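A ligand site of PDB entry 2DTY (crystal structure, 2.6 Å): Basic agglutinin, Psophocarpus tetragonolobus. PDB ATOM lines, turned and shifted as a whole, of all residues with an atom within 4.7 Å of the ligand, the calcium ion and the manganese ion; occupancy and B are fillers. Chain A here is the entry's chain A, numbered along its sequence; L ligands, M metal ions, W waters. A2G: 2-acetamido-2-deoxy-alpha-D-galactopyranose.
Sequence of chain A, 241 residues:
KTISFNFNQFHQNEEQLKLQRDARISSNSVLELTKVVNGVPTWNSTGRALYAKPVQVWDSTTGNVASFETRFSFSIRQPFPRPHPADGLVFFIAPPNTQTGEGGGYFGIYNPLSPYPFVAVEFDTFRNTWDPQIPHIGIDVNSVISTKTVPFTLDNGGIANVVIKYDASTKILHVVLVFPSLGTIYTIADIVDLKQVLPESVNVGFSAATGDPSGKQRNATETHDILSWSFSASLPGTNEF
Water W3 lies within hydrogen-bond range of the backbone carbonyl oxygen (O) of Gly 105 (2.8 Å) and the indole nitrogen (NE1) of Trp 130 (3.3 Å). Water W5 lies within hydrogen-bond range of O of Val 144, OE1 of Glu 122 and NE1 of Trp 130. Water W4 lies within hydrogen-bond range of O1 of the ligand (3.1 Å) and O of Ser 214 (3.4 Å).
Within 4 Å of the calcium ion: Asp 124, Phe 126, Asn 128 and Asp 131. The nearest printed residue that does not touch the calcium ion is Arg 127 (4.4 Å).
The manganese ion is bound by OD1 of Asp 131 (2.2 Å). The manganese ion is bound by the side-chain carboxylate (OE2) of Glu 122 (2.3 Å). The manganese ion is bound by OD2 of Asp 124 (2.3 Å). NE2 of His 136 is bound to the manganese ion. Water W2 is bound to the manganese ion (2.4 Å). Water W5 binds the manganese ion (2.5 Å). The manganese ion has six donor atoms within binding distance.
NE2 of His 84 touches O6 of the ligand, 3.5 Å away. Gly 104 touches the ligand. Trp 130 touches the ligand. CA of Gly 211 touches O4 of the ligand (3.6 Å). Ser 214 touches the ligand. Gly 215 touches the ligand (CA to O5, 3.6 Å). CB of Ala 220 touches O6 of the ligand, 3.6 Å away. Hydrophobic or aromatic side chains that line the ligand: Phe 126, Trp 130 and Ala 220. Of the 25 residues printed, 12 come within 4 Å of the ligand. The nearest printed residue that does not touch the ligand is Tyr 106 (4.03 Å).
Of the 25 residues printed, 4 come within 4 Å of the manganese ion. The nearest printed residue that does not touch the manganese ion is Ser 146 (4.2 Å).
N of Asp 212 is in hydrogen-bond range of O4 of the ligand. An oxygen (O3) of the ligand lies within hydrogen-bond range of the side-chain amide nitrogen (ND2) of Asn 128 (3.1 Å). An oxygen (O3) of the ligand is in hydrogen-bond range of the side-chain carboxylate of Asp 87, at 2.6 Å. The backbone NH of Gly 105 sits at hydrogen-bond distance from an oxygen (O3) of the ligand, at 2.7 Å.
The backbone NH (N) of Gly 105 is in hydrogen-bond range of the side-chain carboxylate (OD2) of Asp 87 (3.4 Å). The backbone carbonyl oxygen of Asp 131 is in hydrogen-bond range of the guanidinium group of Arg 127, 3.2 Å away. The side-chain carboxylate of Glu 122 is in hydrogen-bond range of the side-chain hydroxyl of Ser 146, 3.4 Å away. The backbone NH (N) of Gly 211 lies within hydrogen-bond range of the backbone carbonyl oxygen (O) of Ala 220 (2.7 Å). OD2 of Asp 212 lies within hydrogen-bond range of OG of Ser 214, at 2.6 Å.
The calcium ion is bound by OD2 of Asp 131 (2.3 Å), O of Phe 126 (2.4 Å), water W1 (2.4 Å), water W3 (2.5 Å), OD1 of Asp 124 (2.5 Å), OD1 of Asn 128 (2.5 Å) and OD2 of Asp 124 (2.6 Å).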
ATOM      1  N   HIS A  84      20.595   4.250 -22.206  1.00  0.00           N
ATOM      2  CA  HIS A  84      19.893   5.494 -21.956  1.00  0.00           C
ATOM      3  C   HIS A  84      18.451   5.270 -21.486  1.00  0.00           C
ATOM      4  O   HIS A  84      17.684   4.558 -22.128  1.00  0.00           O
ATOM      5  CB  HIS A  84      19.866   6.292 -23.248  1.00  0.00           C
ATOM      6  CG  HIS A  84      19.534   5.454 -24.448  1.00  0.00           C
ATOM      7  ND1 HIS A  84      20.502   4.883 -25.236  1.00  0.00           N
ATOM      8  CD2 HIS A  84      18.347   5.038 -24.949  1.00  0.00           C
ATOM      9  CE1 HIS A  84      19.926   4.152 -26.179  1.00  0.00           C
ATOM     10  NE2 HIS A  84      18.619   4.227 -26.021  1.00  0.00           N
ATOM     11  N   ALA A  86      14.406   6.092 -20.566  1.00  0.00           N
ATOM     12  CA  ALA A  86      13.362   6.654 -21.421  1.00  0.00           C
ATOM     13  C   ALA A  86      11.963   6.352 -20.886  1.00  0.00           C
ATOM     14  O   ALA A  86      11.783   5.364 -20.176  1.00  0.00           O
ATOM     15  CB  ALA A  86      13.505   6.098 -22.834  1.00  0.00           C
ATOM     16  N   ASP A  87      10.975   7.201 -21.186  1.00  0.00           N
ATOM     17  CA  ASP A  87      11.133   8.403 -22.006  1.00  0.00           C
ATOM     18  C   ASP A  87      10.836   9.674 -21.190  1.00  0.00           C
ATOM     19  O   ASP A  87      11.325  10.766 -21.495  1.00  0.00           O
ATOM     20  CB  ASP A  87      10.174   8.368 -23.199  1.00  0.00           C
ATOM     21  CG  ASP A  87      10.692   7.538 -24.367  1.00  0.00           C
ATOM     22  OD1 ASP A  87      10.455   6.309 -24.400  1.00  0.00           O
ATOM     23  OD2 ASP A  87      11.353   8.135 -25.244  1.00  0.00           O
ATOM     24  N   GLY A 103       3.293   5.767 -27.887  1.00  0.00           N
ATOM     25  CA  GLY A 103       4.171   5.768 -26.725  1.00  0.00           C
ATOM     26  C   GLY A 103       5.538   6.307 -27.077  1.00  0.00           C
ATOM     27  O   GLY A 103       5.655   7.154 -27.960  1.00  0.00           O
ATOM     28  N   GLY A 104       6.563   5.824 -26.391  1.00  0.00           N
ATOM     29  CA  GLY A 104       7.905   6.288 -26.653  1.00  0.00           C
ATOM     30  C   GLY A 104       8.054   7.780 -26.502  1.00  0.00           C
ATOM     31  O   GLY A 104       7.528   8.368 -25.565  1.00  0.00           O
ATOM     32  N   GLY A 105       8.771   8.399 -27.443  1.00  0.00           N
ATOM     33  CA  GLY A 105       8.995   9.824 -27.401  1.00  0.00           C
ATOM     34  C   GLY A 105       7.745  10.674 -27.420  1.00  0.00           C
ATOM     35  O   GLY A 105       7.807  11.877 -27.194  1.00  0.00           O
ATOM     36  N   TYR A 106       6.590  10.060 -27.691  1.00  0.00           N
ATOM     37  CA  TYR A 106       5.346  10.807 -27.729  1.00  0.00           C
ATOM     38  C   TYR A 106       4.580  10.783 -26.396  1.00  0.00           C
ATOM     39  O   TYR A 106       3.476  11.351 -26.291  1.00  0.00           O
ATOM     40  CB  TYR A 106       4.485  10.309 -28.888  1.00  0.00           C
ATOM     41  CG  TYR A 106       5.118  10.609 -30.247  1.00  0.00           C
ATOM     42  CD1 TYR A 106       5.394  11.921 -30.631  1.00  0.00           C
ATOM     43  CD2 TYR A 106       5.479   9.586 -31.117  1.00  0.00           C
ATOM     44  CE1 TYR A 106       5.998  12.207 -31.852  1.00  0.00           C
ATOM     45  CE2 TYR A 106       6.089   9.861 -32.344  1.00  0.00           C
ATOM     46  CZ  TYR A 106       6.350  11.177 -32.703  1.00  0.00           C
ATOM     47  OH  TYR A 106       6.958  11.456 -33.908  1.00  0.00           O
ATOM     48  N   PHE A 107       5.177  10.151 -25.388  1.00  0.00           N
ATOM     49  CA  PHE A 107       4.616  10.090 -24.031  1.00  0.00           C
ATOM     50  C   PHE A 107       3.183   9.562 -23.902  1.00  0.00           C
ATOM     51  O   PHE A 107       2.615   9.580 -22.814  1.00  0.00           O
ATOM     52  CB  PHE A 107       4.647  11.482 -23.398  1.00  0.00           C
ATOM     53  CG  PHE A 107       5.978  12.161 -23.480  1.00  0.00           C
ATOM     54  CD1 PHE A 107       7.057  11.694 -22.756  1.00  0.00           C
ATOM     55  CD2 PHE A 107       6.126  13.318 -24.232  1.00  0.00           C
ATOM     56  CE1 PHE A 107       8.300  12.373 -22.781  1.00  0.00           C
ATOM     57  CE2 PHE A 107       7.346  13.998 -24.263  1.00  0.00           C
ATOM     58  CZ  PHE A 107       8.433  13.525 -23.537  1.00  0.00           C
ATOM     59  N   GLU A 122       6.295  18.830 -20.017  1.00  0.00           N
ATOM     60  CA  GLU A 122       7.025  17.578 -20.025  1.00  0.00           C
ATOM     61  C   GLU A 122       8.310  17.566 -19.210  1.00  0.00           C
ATOM     62  O   GLU A 122       8.968  18.585 -18.996  1.00  0.00           O
ATOM     63  CB  GLU A 122       7.384  17.194 -21.457  1.00  0.00           C
ATOM     64  CG  GLU A 122       8.448  18.111 -22.043  1.00  0.00           C
ATOM     65  CD  GLU A 122       9.001  17.616 -23.364  1.00  0.00           C
ATOM     66  OE1 GLU A 122       8.242  17.555 -24.358  1.00  0.00           O
ATOM     67  OE2 GLU A 122      10.198  17.295 -23.421  1.00  0.00           O
ATOM     68  N   ASP A 124      11.254  15.382 -19.854  1.00  0.00           N
ATOM     69  CA  ASP A 124      11.877  14.510 -20.849  1.00  0.00           C
ATOM     70  C   ASP A 124      13.220  13.928 -20.444  1.00  0.00           C
ATOM     71  O   ASP A 124      14.159  14.660 -20.173  1.00  0.00           O
ATOM     72  CB  ASP A 124      12.055  15.296 -22.145  1.00  0.00           C
ATOM     73  CG  ASP A 124      12.025  14.418 -23.369  1.00  0.00           C
ATOM     74  OD1 ASP A 124      12.332  13.208 -23.253  1.00  0.00           O
ATOM     75  OD2 ASP A 124      11.690  14.938 -24.453  1.00  0.00           O
ATOM     76  N   PHE A 126      14.687  11.197 -22.394  1.00  0.00           N
ATOM     77  CA  PHE A 126      15.338  10.637 -23.575  1.00  0.00           C
ATOM     78  C   PHE A 126      15.440  11.670 -24.685  1.00  0.00           C
ATOM     79  O   PHE A 126      14.502  12.425 -24.949  1.00  0.00           O
ATOM     80  CB  PHE A 126      14.553   9.449 -24.098  1.00  0.00           C
ATOM     81  CG  PHE A 126      15.152   8.838 -25.319  1.00  0.00           C
ATOM     82  CD1 PHE A 126      16.227   7.962 -25.217  1.00  0.00           C
ATOM     83  CD2 PHE A 126      14.686   9.170 -26.590  1.00  0.00           C
ATOM     84  CE1 PHE A 126      16.829   7.434 -26.357  1.00  0.00           C
ATOM     85  CE2 PHE A 126      15.266   8.646 -27.729  1.00  0.00           C
ATOM     86  CZ  PHE A 126      16.343   7.776 -27.619  1.00  0.00           C
ATOM     87  N   ARG A 127      16.585  11.697 -25.358  1.00  0.00           N
ATOM     88  CA  ARG A 127      16.801  12.655 -26.434  1.00  0.00           C
ATOM     89  C   ARG A 127      16.413  12.151 -27.826  1.00  0.00           C
ATOM     90  O   ARG A 127      17.162  11.398 -28.443  1.00  0.00           O
ATOM     91  CB  ARG A 127      18.263  13.106 -26.436  1.00  0.00           C
ATOM     92  CG  ARG A 127      18.539  14.283 -27.365  1.00  0.00           C
ATOM     93  CD  ARG A 127      19.921  14.881 -27.152  1.00  0.00           C
ATOM     94  NE  ARG A 127      20.112  16.074 -27.985  1.00  0.00           N
ATOM     95  CZ  ARG A 127      21.219  16.803 -28.022  1.00  0.00           C
ATOM     96  NH1 ARG A 127      22.265  16.473 -27.269  1.00  0.00           N
ATOM     97  NH2 ARG A 127      21.284  17.874 -28.794  1.00  0.00           N
ATOM     98  N   ASN A 128      15.251  12.574 -28.318  1.00  0.00           N
ATOM     99  CA  ASN A 128      14.816  12.198 -29.648  1.00  0.00           C
ATOM    100  C   ASN A 128      15.451  13.132 -30.665  1.00  0.00           C
ATOM    101  O   ASN A 128      16.142  14.085 -30.307  1.00  0.00           O
ATOM    102  CB  ASN A 128      13.297  12.286 -29.788  1.00  0.00           C
ATOM    103  CG  ASN A 128      12.579  11.209 -29.024  1.00  0.00           C
ATOM    104  OD1 ASN A 128      12.367  11.343 -27.818  1.00  0.00           O
ATOM    105  ND2 ASN A 128      12.225  10.120 -29.703  1.00  0.00           N
ATOM    106  N   TRP A 130      14.255  15.425 -32.279  1.00  0.00           N
ATOM    107  CA  TRP A 130      13.764  16.794 -32.126  1.00  0.00           C
ATOM    108  C   TRP A 130      14.037  17.426 -30.764  1.00  0.00           C
ATOM    109  O   TRP A 130      13.552  18.528 -30.487  1.00  0.00           O
ATOM    110  CB  TRP A 130      12.255  16.809 -32.378  1.00  0.00           C
ATOM    111  CG  TRP A 130      11.509  15.911 -31.419  1.00  0.00           C
ATOM    112  CD1 TRP A 130      11.260  16.134 -30.092  1.00  0.00           C
ATOM    113  CD2 TRP A 130      10.958  14.615 -31.709  1.00  0.00           C
ATOM    114  NE1 TRP A 130      10.594  15.065 -29.540  1.00  0.00           N
ATOM    115  CE2 TRP A 130      10.401  14.112 -30.505  1.00  0.00           C
ATOM    116  CE3 TRP A 130      10.884  13.820 -32.866  1.00  0.00           C
ATOM    117  CZ2 TRP A 130       9.777  12.863 -30.430  1.00  0.00           C
ATOM    118  CZ3 TRP A 130      10.254  12.565 -32.786  1.00  0.00           C
ATOM    119  CH2 TRP A 130       9.713  12.102 -31.575  1.00  0.00           C
ATOM    120  N   ASP A 131      14.805  16.737 -29.918  1.00  0.00           N
ATOM    121  CA  ASP A 131      15.112  17.207 -28.558  1.00  0.00           C
ATOM    122  C   ASP A 131      16.487  17.777 -28.348  1.00  0.00           C
ATOM    123  O   ASP A 131      17.427  17.450 -29.070  1.00  0.00           O
ATOM    124  CB  ASP A 131      15.014  16.063 -27.535  1.00  0.00           C
ATOM    125  CG  ASP A 131      13.601  15.690 -27.170  1.00  0.00           C
ATOM    126  OD1 ASP A 131      12.767  16.597 -27.021  1.00  0.00           O
ATOM    127  OD2 ASP A 131      13.334  14.478 -27.011  1.00  0.00           O
ATOM    128  N   HIS A 136      15.200  17.577 -19.558  1.00  0.00           N
ATOM    129  CA  HIS A 136      14.776  18.952 -19.680  1.00  0.00           C
ATOM    130  C   HIS A 136      13.281  19.106 -19.442  1.00  0.00           C
ATOM    131  O   HIS A 136      12.509  18.177 -19.637  1.00  0.00           O
ATOM    132  CB  HIS A 136      15.159  19.527 -21.059  1.00  0.00           C
ATOM    133  CG  HIS A 136      14.592  18.774 -22.221  1.00  0.00           C
ATOM    134  ND1 HIS A 136      15.361  17.970 -23.041  1.00  0.00           N
ATOM    135  CD2 HIS A 136      13.333  18.710 -22.727  1.00  0.00           C
ATOM    136  CE1 HIS A 136      14.612  17.462 -24.002  1.00  0.00           C
ATOM    137  NE2 HIS A 136      13.376  17.885 -23.832  1.00  0.00           N
ATOM    138  N   VAL A 144       4.985  17.565 -29.551  1.00  0.00           N
ATOM    139  CA  VAL A 144       5.975  17.157 -28.576  1.00  0.00           C
ATOM    140  C   VAL A 144       7.276  17.902 -28.816  1.00  0.00           C
ATOM    141  O   VAL A 144       8.271  17.673 -28.129  1.00  0.00           O
ATOM    142  CB  VAL A 144       6.195  15.649 -28.636  1.00  0.00           C
ATOM    143  CG1 VAL A 144       7.043  15.286 -29.846  1.00  0.00           C
ATOM    144  CG2 VAL A 144       6.817  15.175 -27.346  1.00  0.00           C
ATOM    145  N   SER A 146       8.742  20.992 -28.149  1.00  0.00           N
ATOM    146  CA  SER A 146       8.598  22.139 -27.241  1.00  0.00           C
ATOM    147  C   SER A 146       8.830  23.539 -27.757  1.00  0.00           C
ATOM    148  O   SER A 146       9.682  23.767 -28.598  1.00  0.00           O
ATOM    149  CB  SER A 146       9.512  21.924 -26.033  1.00  0.00           C
ATOM    150  OG  SER A 146       9.300  20.632 -25.483  1.00  0.00           O
ATOM    151  N   THR A 210       7.824   4.393 -21.410  1.00  0.00           N
ATOM    152  CA  THR A 210       9.174   3.859 -21.329  1.00  0.00           C
ATOM    153  C   THR A 210       9.648   3.506 -22.735  1.00  0.00           C
ATOM    154  O   THR A 210       8.886   3.628 -23.689  1.00  0.00           O
ATOM    155  CB  THR A 210       9.250   2.598 -20.406  1.00  0.00           C
ATOM    156  OG1 THR A 210       8.310   1.599 -20.855  1.00  0.00           O
ATOM    157  CG2 THR A 210       8.947   2.993 -18.958  1.00  0.00           C
ATOM    158  N   GLY A 211      10.903   3.097 -22.834  1.00  0.00           N
ATOM    159  CA  GLY A 211      11.502   2.762 -24.124  1.00  0.00           C
ATOM    160  C   GLY A 211      10.623   1.986 -25.086  1.00  0.00           C
ATOM    161  O   GLY A 211      10.002   0.991 -24.716  1.00  0.00           O
ATOM    162  N   ASP A 212      10.571   2.451 -26.325  1.00  0.00           N
ATOM    163  CA  ASP A 212       9.783   1.784 -27.344  1.00  0.00           C
ATOM    164  C   ASP A 212      10.594   0.607 -27.919  1.00  0.00           C
ATOM    165  O   ASP A 212      11.818   0.690 -28.039  1.00  0.00           O
ATOM    166  CB  ASP A 212       9.436   2.763 -28.468  1.00  0.00           C
ATOM    167  CG  ASP A 212       8.588   2.115 -29.546  1.00  0.00           C
ATOM    168  OD1 ASP A 212       7.419   1.763 -29.253  1.00  0.00           O
ATOM    169  OD2 ASP A 212       9.084   1.966 -30.676  1.00  0.00           O
ATOM    170  N   SER A 214      11.052  -0.495 -30.868  1.00  0.00           N
ATOM    171  CA  SER A 214      11.813  -0.138 -32.063  1.00  0.00           C
ATOM    172  C   SER A 214      13.244   0.282 -31.745  1.00  0.00           C
ATOM    173  O   SER A 214      14.134   0.193 -32.597  1.00  0.00           O
ATOM    174  CB  SER A 214      11.118   0.992 -32.824  1.00  0.00           C
ATOM    175  OG  SER A 214      11.219   2.225 -32.116  1.00  0.00           O
ATOM    176  N   GLY A 215      13.463   0.758 -30.526  1.00  0.00           N
ATOM    177  CA  GLY A 215      14.790   1.200 -30.124  1.00  0.00           C
ATOM    178  C   GLY A 215      15.725   0.045 -29.843  1.00  0.00           C
ATOM    179  O   GLY A 215      16.943   0.237 -29.752  1.00  0.00           O
ATOM    180  N   GLN A 217      16.192  -1.744 -27.102  1.00  0.00           N
ATOM    181  CA  GLN A 217      16.903  -1.614 -25.838  1.00  0.00           C
ATOM    182  C   GLN A 217      15.970  -1.759 -24.653  1.00  0.00           C
ATOM    183  O   GLN A 217      15.212  -0.850 -24.330  1.00  0.00           O
ATOM    184  CB  GLN A 217      17.608  -0.249 -25.788  1.00  0.00           C
ATOM    185  CG  GLN A 217      18.807  -0.167 -26.691  1.00  0.00           C
ATOM    186  CD  GLN A 217      19.907  -1.114 -26.257  1.00  0.00           C
ATOM    187  OE1 GLN A 217      20.813  -1.416 -27.023  1.00  0.00           O
ATOM    188  NE2 GLN A 217      19.847  -1.571 -24.996  1.00  0.00           N
ATOM    189  N   ALA A 220      16.195   0.776 -21.840  1.00  0.00           N
ATOM    190  CA  ALA A 220      15.633   2.117 -22.016  1.00  0.00           C
ATOM    191  C   ALA A 220      14.318   2.214 -21.249  1.00  0.00           C
ATOM    192  O   ALA A 220      13.235   2.215 -21.828  1.00  0.00           O
ATOM    193  CB  ALA A 220      15.428   2.414 -23.498  1.00  0.00           C
HETATM  194  O5  A2G L   1      13.270   4.193 -28.890  1.00  0.00           O
HETATM  195  C1  A2G L   1      12.814   5.049 -30.030  1.00  0.00           C
HETATM  196  O1  A2G L   1      13.902   5.738 -30.668  1.00  0.00           O
HETATM  197  C2  A2G L   1      11.748   6.084 -29.495  1.00  0.00           C
HETATM  198  N2  A2G L   1      11.312   6.950 -30.585  1.00  0.00           N
HETATM  199  C3  A2G L   1      12.377   6.912 -28.311  1.00  0.00           C
HETATM  200  O3  A2G L   1      11.426   7.848 -27.826  1.00  0.00           O
HETATM  201  C4  A2G L   1      12.812   5.952 -27.184  1.00  0.00           C
HETATM  202  O4  A2G L   1      11.675   5.268 -26.647  1.00  0.00           O
HETATM  203  C5  A2G L   1      13.839   4.941 -27.749  1.00  0.00           C
HETATM  204  C6  A2G L   1      14.287   3.944 -26.687  1.00  0.00           C
HETATM  205  O6  A2G L   1      15.429   3.167 -27.067  1.00  0.00           O
HETATM  206  C7  A2G L   1      10.017   7.260 -30.790  1.00  0.00           C
HETATM  207  O7  A2G L   1       9.082   6.854 -30.092  1.00  0.00           O
HETATM  208  C8  A2G L   1       9.731   8.186 -31.967  1.00  0.00           C
HETATM  209 CA    CA M   1      12.295  12.799 -25.741  1.00  0.00          CA
HETATM  210 MN    MN M   2      11.615  17.149 -25.191  1.00  0.00          MN
HETATM  211  O   HOH W   1      11.102  10.904 -24.804  1.00  0.00           O
HETATM  212  O   HOH W   2      11.381  19.180 -26.357  1.00  0.00           O
HETATM  213  O   HOH W   3      10.092  13.345 -26.719  1.00  0.00           O
HETATM  214  O   HOH W   4      14.635   3.519 -32.726  1.00  0.00           O
HETATM  215  O   HOH W   5       9.708  16.094 -26.367  1.00  0.00           O
